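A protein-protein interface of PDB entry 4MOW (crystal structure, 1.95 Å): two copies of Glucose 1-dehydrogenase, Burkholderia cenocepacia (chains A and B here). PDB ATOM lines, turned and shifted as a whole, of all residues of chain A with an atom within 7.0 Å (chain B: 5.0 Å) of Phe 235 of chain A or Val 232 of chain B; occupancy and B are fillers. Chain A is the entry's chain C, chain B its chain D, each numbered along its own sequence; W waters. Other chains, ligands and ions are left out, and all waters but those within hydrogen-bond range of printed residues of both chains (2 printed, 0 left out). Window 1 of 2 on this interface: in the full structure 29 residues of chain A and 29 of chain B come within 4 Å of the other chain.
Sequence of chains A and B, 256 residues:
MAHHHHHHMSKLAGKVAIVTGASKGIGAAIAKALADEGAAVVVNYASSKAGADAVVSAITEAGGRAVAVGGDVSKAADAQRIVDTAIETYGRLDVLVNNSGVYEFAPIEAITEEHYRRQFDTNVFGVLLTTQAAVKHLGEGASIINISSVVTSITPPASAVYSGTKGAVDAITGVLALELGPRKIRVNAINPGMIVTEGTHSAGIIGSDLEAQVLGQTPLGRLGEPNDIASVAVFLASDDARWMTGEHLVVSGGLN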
ATOM      1  N   LYS A  11     -21.926 -32.489 -16.730  1.00  0.00           N
ATOM      2  CA  LYS A  11     -23.200 -32.352 -17.419  1.00  0.00           C
ATOM      3  C   LYS A  11     -23.808 -33.657 -17.948  1.00  0.00           C
ATOM      4  O   LYS A  11     -25.010 -33.724 -18.126  1.00  0.00           O
ATOM      5  CB  LYS A  11     -23.032 -31.341 -18.548  1.00  0.00           C
ATOM      6  CG  LYS A  11     -22.725 -29.953 -18.022  1.00  0.00           C
ATOM      7  CD  LYS A  11     -22.352 -28.987 -19.144  1.00  0.00           C
ATOM      8  CE  LYS A  11     -21.966 -27.601 -18.601  1.00  0.00           C
ATOM      9  NZ  LYS A  11     -23.016 -26.967 -17.748  1.00  0.00           N
ATOM     10  N   LEU A  34     -17.337 -34.776 -24.968  1.00  0.00           N
ATOM     11  CA  LEU A  34     -18.487 -35.410 -24.308  1.00  0.00           C
ATOM     12  C   LEU A  34     -17.979 -36.230 -23.113  1.00  0.00           C
ATOM     13  O   LEU A  34     -18.566 -36.229 -22.044  1.00  0.00           O
ATOM     14  CB  LEU A  34     -19.298 -36.299 -25.259  1.00  0.00           C
ATOM     15  CG  LEU A  34     -20.039 -35.573 -26.395  1.00  0.00           C
ATOM     16  CD1 LEU A  34     -20.620 -36.594 -27.332  1.00  0.00           C
ATOM     17  CD2 LEU A  34     -21.127 -34.676 -25.868  1.00  0.00           C
ATOM     18  N   SER A 143     -30.786 -36.589 -26.786  1.00  0.00           N
ATOM     19  CA  SER A 143     -30.398 -35.486 -27.663  1.00  0.00           C
ATOM     20  C   SER A 143     -29.669 -36.033 -28.877  1.00  0.00           C
ATOM     21  O   SER A 143     -28.671 -36.710 -28.750  1.00  0.00           O
ATOM     22  CB  SER A 143     -29.490 -34.560 -26.910  1.00  0.00           C
ATOM     23  OG  SER A 143     -29.125 -33.443 -27.714  1.00  0.00           O
ATOM     24  N   ILE A 145     -27.789 -34.845 -32.368  1.00  0.00           N
ATOM     25  CA  ILE A 145     -27.062 -33.679 -32.903  1.00  0.00           C
ATOM     26  C   ILE A 145     -26.593 -34.037 -34.295  1.00  0.00           C
ATOM     27  O   ILE A 145     -25.818 -34.983 -34.479  1.00  0.00           O
ATOM     28  CB  ILE A 145     -25.874 -33.304 -31.992  1.00  0.00           C
ATOM     29  CG1 ILE A 145     -26.402 -32.972 -30.568  1.00  0.00           C
ATOM     30  CG2 ILE A 145     -25.139 -32.127 -32.594  1.00  0.00           C
ATOM     31  CD1 ILE A 145     -25.383 -33.125 -29.473  1.00  0.00           C
ATOM     32  N   ARG A 186     -34.793 -34.391 -28.124  1.00  0.00           N
ATOM     33  CA  ARG A 186     -34.359 -33.187 -28.863  1.00  0.00           C
ATOM     34  C   ARG A 186     -33.500 -33.554 -30.073  1.00  0.00           C
ATOM     35  O   ARG A 186     -32.691 -34.511 -30.053  1.00  0.00           O
ATOM     36  CB  ARG A 186     -33.589 -32.244 -27.919  1.00  0.00           C
ATOM     37  CG  ARG A 186     -34.483 -31.742 -26.784  1.00  0.00           C
ATOM     38  CD  ARG A 186     -33.835 -30.734 -25.862  1.00  0.00           C
ATOM     39  NE  ARG A 186     -32.711 -31.362 -25.185  1.00  0.00           N
ATOM     40  CZ  ARG A 186     -31.428 -31.176 -25.465  1.00  0.00           C
ATOM     41  NH1 ARG A 186     -31.016 -30.343 -26.465  1.00  0.00           N
ATOM     42  NH2 ARG A 186     -30.523 -31.861 -24.772  1.00  0.00           N
ATOM     43  N   ALA A 230     -16.829 -28.910 -31.042  1.00  0.00           N
ATOM     44  CA  ALA A 230     -17.011 -29.774 -29.903  1.00  0.00           C
ATOM     45  C   ALA A 230     -17.774 -29.117 -28.748  1.00  0.00           C
ATOM     46  O   ALA A 230     -18.707 -29.712 -28.210  1.00  0.00           O
ATOM     47  CB  ALA A 230     -15.674 -30.346 -29.430  1.00  0.00           C
ATOM     48  N   SER A 231     -17.403 -27.901 -28.379  1.00  0.00           N
ATOM     49  CA  SER A 231     -18.028 -27.216 -27.245  1.00  0.00           C
ATOM     50  C   SER A 231     -19.510 -26.960 -27.478  1.00  0.00           C
ATOM     51  O   SER A 231     -20.313 -27.016 -26.556  1.00  0.00           O
ATOM     52  CB  SER A 231     -17.255 -25.964 -26.844  1.00  0.00           C
ATOM     53  OG  SER A 231     -17.275 -24.979 -27.846  1.00  0.00           O
ATOM     54  N   VAL A 232     -19.897 -26.772 -28.735  1.00  0.00           N
ATOM     55  CA  VAL A 232     -21.293 -26.552 -29.045  1.00  0.00           C
ATOM     56  C   VAL A 232     -22.067 -27.863 -28.992  1.00  0.00           C
ATOM     57  O   VAL A 232     -23.203 -27.898 -28.524  1.00  0.00           O
ATOM     58  CB  VAL A 232     -21.469 -25.860 -30.403  1.00  0.00           C
ATOM     59  CG1 VAL A 232     -22.929 -25.622 -30.663  1.00  0.00           C
ATOM     60  CG2 VAL A 232     -20.656 -24.569 -30.477  1.00  0.00           C
ATOM     61  N   ALA A 233     -21.450 -28.934 -29.425  1.00  0.00           N
ATOM     62  CA  ALA A 233     -22.098 -30.242 -29.365  1.00  0.00           C
ATOM     63  C   ALA A 233     -22.369 -30.625 -27.888  1.00  0.00           C
ATOM     64  O   ALA A 233     -23.402 -31.180 -27.564  1.00  0.00           O
ATOM     65  CB  ALA A 233     -21.208 -31.292 -29.999  1.00  0.00           C
ATOM     66  N   VAL A 234     -21.402 -30.344 -27.022  1.00  0.00           N
ATOM     67  CA  VAL A 234     -21.569 -30.639 -25.586  1.00  0.00           C
ATOM     68  C   VAL A 234     -22.779 -29.868 -25.021  1.00  0.00           C
ATOM     69  O   VAL A 234     -23.671 -30.477 -24.380  1.00  0.00           O
ATOM     70  CB  VAL A 234     -20.269 -30.356 -24.816  1.00  0.00           C
ATOM     71  CG1 VAL A 234     -20.467 -30.512 -23.311  1.00  0.00           C
ATOM     72  CG2 VAL A 234     -19.216 -31.357 -25.272  1.00  0.00           C
ATOM     73  N   PHE A 235     -22.810 -28.557 -25.259  1.00  0.00           N
ATOM     74  CA  PHE A 235     -23.957 -27.724 -24.905  1.00  0.00           C
ATOM     75  C   PHE A 235     -25.270 -28.392 -25.382  1.00  0.00           C
ATOM     76  O   PHE A 235     -26.143 -28.671 -24.559  1.00  0.00           O
ATOM     77  CB  PHE A 235     -23.821 -26.291 -25.475  1.00  0.00           C
ATOM     78  CG  PHE A 235     -25.120 -25.534 -25.540  1.00  0.00           C
ATOM     79  CD1 PHE A 235     -25.756 -25.103 -24.380  1.00  0.00           C
ATOM     80  CD2 PHE A 235     -25.744 -25.292 -26.759  1.00  0.00           C
ATOM     81  CE1 PHE A 235     -26.952 -24.425 -24.441  1.00  0.00           C
ATOM     82  CE2 PHE A 235     -26.928 -24.585 -26.818  1.00  0.00           C
ATOM     83  CZ  PHE A 235     -27.542 -24.156 -25.663  1.00  0.00           C
ATOM     84  N   LEU A 236     -25.367 -28.746 -26.678  1.00  0.00           N
ATOM     85  CA  LEU A 236     -26.625 -29.306 -27.203  1.00  0.00           C
ATOM     86  C   LEU A 236     -26.937 -30.667 -26.632  1.00  0.00           C
ATOM     87  O   LEU A 236     -28.112 -31.042 -26.581  1.00  0.00           O
ATOM     88  CB  LEU A 236     -26.571 -29.469 -28.744  1.00  0.00           C
ATOM     89  CG  LEU A 236     -26.599 -28.131 -29.529  1.00  0.00           C
ATOM     90  CD1 LEU A 236     -26.340 -28.367 -31.014  1.00  0.00           C
ATOM     91  CD2 LEU A 236     -27.941 -27.459 -29.397  1.00  0.00           C
ATOM     92  N   ALA A 237     -25.894 -31.429 -26.292  1.00  0.00           N
ATOM     93  CA  ALA A 237     -26.096 -32.736 -25.698  1.00  0.00           C
ATOM     94  C   ALA A 237     -26.648 -32.679 -24.284  1.00  0.00           C
ATOM     95  O   ALA A 237     -27.317 -33.630 -23.829  1.00  0.00           O
ATOM     96  CB  ALA A 237     -24.815 -33.521 -25.696  1.00  0.00           C
ATOM     97  N   SER A 238     -26.329 -31.587 -23.598  1.00  0.00           N
ATOM     98  CA  SER A 238     -26.570 -31.411 -22.160  1.00  0.00           C
ATOM     99  C   SER A 238     -27.983 -30.818 -21.902  1.00  0.00           C
ATOM    100  O   SER A 238     -28.596 -30.265 -22.806  1.00  0.00           O
ATOM    101  CB  SER A 238     -25.560 -30.397 -21.629  1.00  0.00           C
ATOM    102  OG  SER A 238     -26.014 -29.045 -21.916  1.00  0.00           O
ATOM    103  N   ASP A 239     -28.391 -30.812 -20.620  1.00  0.00           N
ATOM    104  CA  ASP A 239     -29.660 -30.264 -20.164  1.00  0.00           C
ATOM    105  C   ASP A 239     -29.708 -28.746 -20.289  1.00  0.00           C
ATOM    106  O   ASP A 239     -30.788 -28.129 -20.139  1.00  0.00           O
ATOM    107  CB  ASP A 239     -29.902 -30.736 -18.700  1.00  0.00           C
ATOM    108  CG  ASP A 239     -31.266 -30.356 -18.138  1.00  0.00           C
ATOM    109  OD1 ASP A 239     -32.317 -30.753 -18.715  1.00  0.00           O
ATOM    110  OD2 ASP A 239     -31.307 -29.698 -17.053  1.00  0.00           O
ATOM    111  N   ASP A 240     -28.555 -28.137 -20.585  1.00  0.00           N
ATOM    112  CA  ASP A 240     -28.490 -26.687 -20.792  1.00  0.00           C
ATOM    113  C   ASP A 240     -29.314 -26.270 -22.028  1.00  0.00           C
ATOM    114  O   ASP A 240     -29.864 -25.155 -22.080  1.00  0.00           O
ATOM    115  CB  ASP A 240     -27.042 -26.189 -20.913  1.00  0.00           C
ATOM    116  CG  ASP A 240     -26.266 -26.270 -19.570  1.00  0.00           C
ATOM    117  OD1 ASP A 240     -26.950 -26.374 -18.559  1.00  0.00           O
ATOM    118  OD2 ASP A 240     -24.999 -26.221 -19.545  1.00  0.00           O
ATOM    119  N   ALA A 241     -29.456 -27.214 -22.958  1.00  0.00           N
ATOM    120  CA  ALA A 241     -30.233 -27.011 -24.190  1.00  0.00           C
ATOM    121  C   ALA A 241     -31.618 -27.708 -24.155  1.00  0.00           C
ATOM    122  O   ALA A 241     -32.197 -28.010 -25.208  1.00  0.00           O
ATOM    123  CB  ALA A 241     -29.424 -27.541 -25.392  1.00  0.00           C
ATOM    124  N   ARG A 242     -32.156 -27.961 -22.968  1.00  0.00           N
ATOM    125  CA  ARG A 242     -33.405 -28.748 -22.833  1.00  0.00           C
ATOM    126  C   ARG A 242     -34.614 -28.104 -23.477  1.00  0.00           C
ATOM    127  O   ARG A 242     -35.582 -28.797 -23.809  1.00  0.00           O
ATOM    128  CB  ARG A 242     -33.727 -29.022 -21.359  1.00  0.00           C
ATOM    129  CG  ARG A 242     -34.096 -27.822 -20.594  1.00  0.00           C
ATOM    130  CD  ARG A 242     -34.006 -28.141 -19.088  1.00  0.00           C
ATOM    131  NE  ARG A 242     -34.192 -26.968 -18.318  1.00  0.00           N
ATOM    132  CZ  ARG A 242     -33.285 -26.008 -18.131  1.00  0.00           C
ATOM    133  NH1 ARG A 242     -32.055 -26.057 -18.632  1.00  0.00           N
ATOM    134  NH2 ARG A 242     -33.616 -24.981 -17.369  1.00  0.00           N
ATOM    135  N   TRP A 243     -34.550 -26.785 -23.684  1.00  0.00           N
ATOM    136  CA  TRP A 243     -35.610 -26.071 -24.329  1.00  0.00           C
ATOM    137  C   TRP A 243     -35.361 -25.651 -25.801  1.00  0.00           C
ATOM    138  O   TRP A 243     -36.134 -24.853 -26.348  1.00  0.00           O
ATOM    139  CB  TRP A 243     -36.031 -24.878 -23.428  1.00  0.00           C
ATOM    140  CG  TRP A 243     -37.505 -24.487 -23.590  1.00  0.00           C
ATOM    141  CD1 TRP A 243     -38.022 -23.226 -23.795  1.00  0.00           C
ATOM    142  CD2 TRP A 243     -38.600 -25.356 -23.489  1.00  0.00           C
ATOM    143  NE1 TRP A 243     -39.372 -23.294 -23.877  1.00  0.00           N
ATOM    144  CE2 TRP A 243     -39.748 -24.606 -23.703  1.00  0.00           C
ATOM    145  CE3 TRP A 243     -38.719 -26.740 -23.273  1.00  0.00           C
ATOM    146  CZ2 TRP A 243     -41.004 -25.176 -23.750  1.00  0.00           C
ATOM    147  CZ3 TRP A 243     -39.986 -27.303 -23.288  1.00  0.00           C
ATOM    148  CH2 TRP A 243     -41.100 -26.530 -23.525  1.00  0.00           C
ATOM    149  N   MET A 244     -34.365 -26.266 -26.439  1.00  0.00           N
ATOM    150  CA  MET A 244     -34.079 -26.096 -27.834  1.00  0.00           C
ATOM    151  C   MET A 244     -34.226 -27.405 -28.595  1.00  0.00           C
ATOM    152  O   MET A 244     -33.625 -28.392 -28.253  1.00  0.00           O
ATOM    153  CB  MET A 244     -32.639 -25.621 -28.049  1.00  0.00           C
ATOM    154  CG  MET A 244     -32.353 -24.268 -27.491  1.00  0.00           C
ATOM    155  SD  MET A 244     -30.642 -23.661 -27.752  1.00  0.00           S
ATOM    156  CE  MET A 244     -30.448 -23.989 -29.449  1.00  0.00           C
ATOM    157  N   LEU A 249     -27.411 -24.369 -35.456  1.00  0.00           N
ATOM    158  CA  LEU A 249     -26.524 -23.384 -34.911  1.00  0.00           C
ATOM    159  C   LEU A 249     -25.350 -23.230 -35.864  1.00  0.00           C
ATOM    160  O   LEU A 249     -24.630 -24.199 -36.079  1.00  0.00           O
ATOM    161  CB  LEU A 249     -26.021 -23.832 -33.561  1.00  0.00           C
ATOM    162  CG  LEU A 249     -26.943 -23.575 -32.403  1.00  0.00           C
ATOM    163  CD1 LEU A 249     -28.217 -24.384 -32.552  1.00  0.00           C
ATOM    164  CD2 LEU A 249     -26.284 -24.021 -31.112  1.00  0.00           C
ATOM    165  N   ILE B 190     -30.841 -14.584 -28.121  1.00  0.00           N
ATOM    166  CA  ILE B 190     -31.769 -15.659 -27.774  1.00  0.00           C
ATOM    167  C   ILE B 190     -33.162 -15.192 -28.149  1.00  0.00           C
ATOM    168  O   ILE B 190     -33.568 -13.988 -27.917  1.00  0.00           O
ATOM    169  CB  ILE B 190     -31.665 -16.032 -26.280  1.00  0.00           C
ATOM    170  CG1 ILE B 190     -30.218 -16.414 -25.924  1.00  0.00           C
ATOM    171  CG2 ILE B 190     -32.613 -17.175 -25.923  1.00  0.00           C
ATOM    172  CD1 ILE B 190     -29.932 -16.470 -24.447  1.00  0.00           C
ATOM    173  N   ASP B 228     -34.843 -22.179 -18.488  1.00  0.00           N
ATOM    174  CA  ASP B 228     -34.669 -22.684 -19.862  1.00  0.00           C
ATOM    175  C   ASP B 228     -33.913 -21.655 -20.711  1.00  0.00           C
ATOM    176  O   ASP B 228     -33.194 -22.023 -21.629  1.00  0.00           O
ATOM    177  CB  ASP B 228     -36.007 -22.949 -20.521  1.00  0.00           C
ATOM    178  CG  ASP B 228     -36.760 -24.104 -19.908  1.00  0.00           C
ATOM    179  OD1 ASP B 228     -36.147 -25.160 -19.553  1.00  0.00           O
ATOM    180  OD2 ASP B 228     -38.014 -23.943 -19.823  1.00  0.00           O
ATOM    181  N   ILE B 229     -34.110 -20.368 -20.452  1.00  0.00           N
ATOM    182  CA  ILE B 229     -33.386 -19.305 -21.167  1.00  0.00           C
ATOM    183  C   ILE B 229     -32.028 -19.057 -20.528  1.00  0.00           C
ATOM    184  O   ILE B 229     -31.006 -18.873 -21.200  1.00  0.00           O
ATOM    185  CB  ILE B 229     -34.221 -18.014 -21.212  1.00  0.00           C
ATOM    186  CG1 ILE B 229     -35.645 -18.281 -21.766  1.00  0.00           C
ATOM    187  CG2 ILE B 229     -33.519 -16.930 -21.996  1.00  0.00           C
ATOM    188  CD1 ILE B 229     -35.712 -19.136 -23.043  1.00  0.00           C
ATOM    189  N   ALA B 230     -32.008 -19.056 -19.195  1.00  0.00           N
ATOM    190  CA  ALA B 230     -30.779 -18.759 -18.474  1.00  0.00           C
ATOM    191  C   ALA B 230     -29.592 -19.630 -18.870  1.00  0.00           C
ATOM    192  O   ALA B 230     -28.462 -19.161 -19.051  1.00  0.00           O
ATOM    193  CB  ALA B 230     -31.032 -18.854 -16.936  1.00  0.00           C
ATOM    194  N   SER B 231     -29.830 -20.923 -18.961  1.00  0.00           N
ATOM    195  CA  SER B 231     -28.743 -21.820 -19.279  1.00  0.00           C
ATOM    196  C   SER B 231     -28.161 -21.558 -20.721  1.00  0.00           C
ATOM    197  O   SER B 231     -26.957 -21.697 -20.968  1.00  0.00           O
ATOM    198  CB  SER B 231     -29.196 -23.248 -19.046  1.00  0.00           C
ATOM    199  OG  SER B 231     -30.205 -23.600 -19.982  1.00  0.00           O
ATOM    200  N   VAL B 232     -29.000 -21.122 -21.646  1.00  0.00           N
ATOM    201  CA  VAL B 232     -28.521 -20.772 -22.996  1.00  0.00           C
ATOM    202  C   VAL B 232     -27.716 -19.470 -22.948  1.00  0.00           C
ATOM    203  O   VAL B 232     -26.772 -19.272 -23.692  1.00  0.00           O
ATOM    204  CB  VAL B 232     -29.706 -20.667 -23.964  1.00  0.00           C
ATOM    205  CG1 VAL B 232     -29.234 -20.254 -25.336  1.00  0.00           C
ATOM    206  CG2 VAL B 232     -30.460 -21.988 -24.041  1.00  0.00           C
ATOM    207  N   ALA B 233     -28.104 -18.542 -22.081  1.00  0.00           N
ATOM    208  CA  ALA B 233     -27.343 -17.293 -21.945  1.00  0.00           C
ATOM    209  C   ALA B 233     -25.927 -17.563 -21.434  1.00  0.00           C
ATOM    210  O   ALA B 233     -24.950 -16.926 -21.865  1.00  0.00           O
ATOM    211  CB  ALA B 233     -28.076 -16.332 -20.977  1.00  0.00           C
ATOM    212  N   VAL B 234     -25.829 -18.517 -20.511  1.00  0.00           N
ATOM    213  CA  VAL B 234     -24.535 -18.857 -19.895  1.00  0.00           C
ATOM    214  C   VAL B 234     -23.663 -19.477 -20.983  1.00  0.00           C
ATOM    215  O   VAL B 234     -22.485 -19.170 -21.085  1.00  0.00           O
ATOM    216  CB  VAL B 234     -24.706 -19.865 -18.738  1.00  0.00           C
ATOM    217  CG1 VAL B 234     -23.362 -20.485 -18.330  1.00  0.00           C
ATOM    218  CG2 VAL B 234     -25.334 -19.183 -17.548  1.00  0.00           C
ATOM    219  N   PHE B 235     -24.266 -20.286 -21.852  1.00  0.00           N
ATOM    220  CA  PHE B 235     -23.495 -20.860 -22.961  1.00  0.00           C
ATOM    221  C   PHE B 235     -22.964 -19.740 -23.858  1.00  0.00           C
ATOM    222  O   PHE B 235     -21.755 -19.675 -24.140  1.00  0.00           O
ATOM    223  CB  PHE B 235     -24.346 -21.891 -23.708  1.00  0.00           C
ATOM    224  CG  PHE B 235     -23.884 -22.174 -25.090  1.00  0.00           C
ATOM    225  CD1 PHE B 235     -22.756 -22.927 -25.307  1.00  0.00           C
ATOM    226  CD2 PHE B 235     -24.601 -21.702 -26.181  1.00  0.00           C
ATOM    227  CE1 PHE B 235     -22.312 -23.188 -26.603  1.00  0.00           C
ATOM    228  CE2 PHE B 235     -24.171 -21.944 -27.479  1.00  0.00           C
ATOM    229  CZ  PHE B 235     -23.029 -22.677 -27.708  1.00  0.00           C
ATOM    230  N   LEU B 236     -23.844 -18.833 -24.291  1.00  0.00           N
ATOM    231  CA  LEU B 236     -23.410 -17.747 -25.187  1.00  0.00           C
ATOM    232  C   LEU B 236     -22.409 -16.788 -24.562  1.00  0.00           C
ATOM    233  O   LEU B 236     -21.566 -16.291 -25.276  1.00  0.00           O
ATOM    234  CB  LEU B 236     -24.591 -16.946 -25.717  1.00  0.00           C
ATOM    235  CG  LEU B 236     -25.482 -17.725 -26.667  1.00  0.00           C
ATOM    236  CD1 LEU B 236     -26.730 -16.882 -26.978  1.00  0.00           C
ATOM    237  CD2 LEU B 236     -24.742 -18.141 -27.921  1.00  0.00           C
ATOM    238  N   LEU B 249     -30.782 -17.819 -31.414  1.00  0.00           N
ATOM    239  CA  LEU B 249     -31.105 -19.169 -30.902  1.00  0.00           C
ATOM    240  C   LEU B 249     -32.524 -19.163 -30.439  1.00  0.00           C
ATOM    241  O   LEU B 249     -32.819 -18.546 -29.381  1.00  0.00           O
ATOM    242  CB  LEU B 249     -30.167 -19.584 -29.728  1.00  0.00           C
ATOM    243  CG  LEU B 249     -28.760 -20.106 -30.045  1.00  0.00           C
ATOM    244  CD1 LEU B 249     -27.912 -19.016 -30.685  1.00  0.00           C
ATOM    245  CD2 LEU B 249     -27.998 -20.580 -28.814  1.00  0.00           C
ATOM    246  N   VAL B 251     -35.403 -20.598 -28.407  1.00  0.00           N
ATOM    247  CA  VAL B 251     -35.497 -21.406 -27.210  1.00  0.00           C
ATOM    248  C   VAL B 251     -36.946 -21.407 -26.794  1.00  0.00           C
ATOM    249  O   VAL B 251     -37.346 -20.651 -25.897  1.00  0.00           O
ATOM    250  CB  VAL B 251     -34.558 -20.841 -26.106  1.00  0.00           C
ATOM    251  CG1 VAL B 251     -34.513 -21.794 -24.926  1.00  0.00           C
ATOM    252  CG2 VAL B 251     -33.146 -20.677 -26.630  1.00  0.00           C
HETATM  253  O   HOH W   1     -32.590 -24.656 -22.745  1.00  0.00           O
HETATM  254  O   HOH W   2     -25.202 -23.265 -19.692  1.00  0.00           O
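Of the printed residues of chain B, Phe 235 of chain A touches Val 232 (3.98 Å) and Phe 235 (3.5 Å).
Printed residues of chain B within 4 Å of Asp 240 of chain A: Ser 231 and Val 232.
Ala 241 of chain A touches none of the printed residues of chain B.
Of the printed residues of chain B, Trp 243 of chain A touches Asp 228 and Val 251.
Printed residues of chain A within 4 Å of Asp 228 of chain B: Arg 242 and Trp 243.
Of the printed residues of chain A, Phe 235 of chain B touches Phe 235.
The nearest printed residue of chain A that does not touch Val 232 of chain B is Met 244 of chain A (4.1 Å).
O of Asp 240 of chain A sits at hydrogen-bond distance from OG of Ser 231 of chain B, 2.6 Å away.
NE of Arg 242 of chain A is in salt-bridge range of OD1 of Asp 228 of chain B, 2.9 Å away.
The guanidinium group (NH1) of Arg 242 of chain A sits at hydrogen-bond distance from the side-chain hydroxyl (OG) of Ser 231 of chain B.
Among the printed residues, merely in contact across the chains: Phe 235 of chain A with Val 232 of chain B, Phe 235 of chain A with Phe 235 of chain B, Asp 240 of chain A with Val 232 of chain B, Trp 243 of chain A with Asp 228 of chain B, Trp 243 of chain A with Val 251 of chain B and Met 244 of chain A with Val 251 of chain B.
Phe 235 of chain A touches Val 232 of chain B, but with the chains exchanged Val 232 of chain A does not touch Phe 235 of chain B (4.1 Å).
Phe 235 of chain A touches its own counterpart, Phe 235 of chain B.
Positions printed for both chains: 230, 231, 232, 233, 234, 235, 236 and 249.
Of the 9 pairs that touch across the chains among the printed residues, 1 has its exchanged pair printed and touching as well.
NZ of Lys 11 of chain A is in salt-bridge range of OD2 of Asp 240 of chain A, at 2.8 Å.
OG of Ser 238 of chain A is in hydrogen-bond range of O of Phe 235 of chain A (2.7 Å).
The side-chain hydroxyl of Ser 238 of chain A lies within hydrogen-bond range of the backbone NH of Asp 240 of chain A.
NH1 of Arg 242 of chain A lies within hydrogen-bond range of O of Asp 239 of chain A (2.9 Å).
Water W2 bridges the backbone carbonyl oxygen of Ser 231 of chain B (2.7 Å) and the side-chain carboxylate of Asp 240 of chain A (3.0 Å).
Water W1 lies within hydrogen-bond range of O of Asp 240 of chain A (2.8 Å), O of Asp 228 of chain B (2.9 Å), N of Trp 243 of chain A (3.0 Å) and N of Arg 242 of chain A (3.3 Å).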
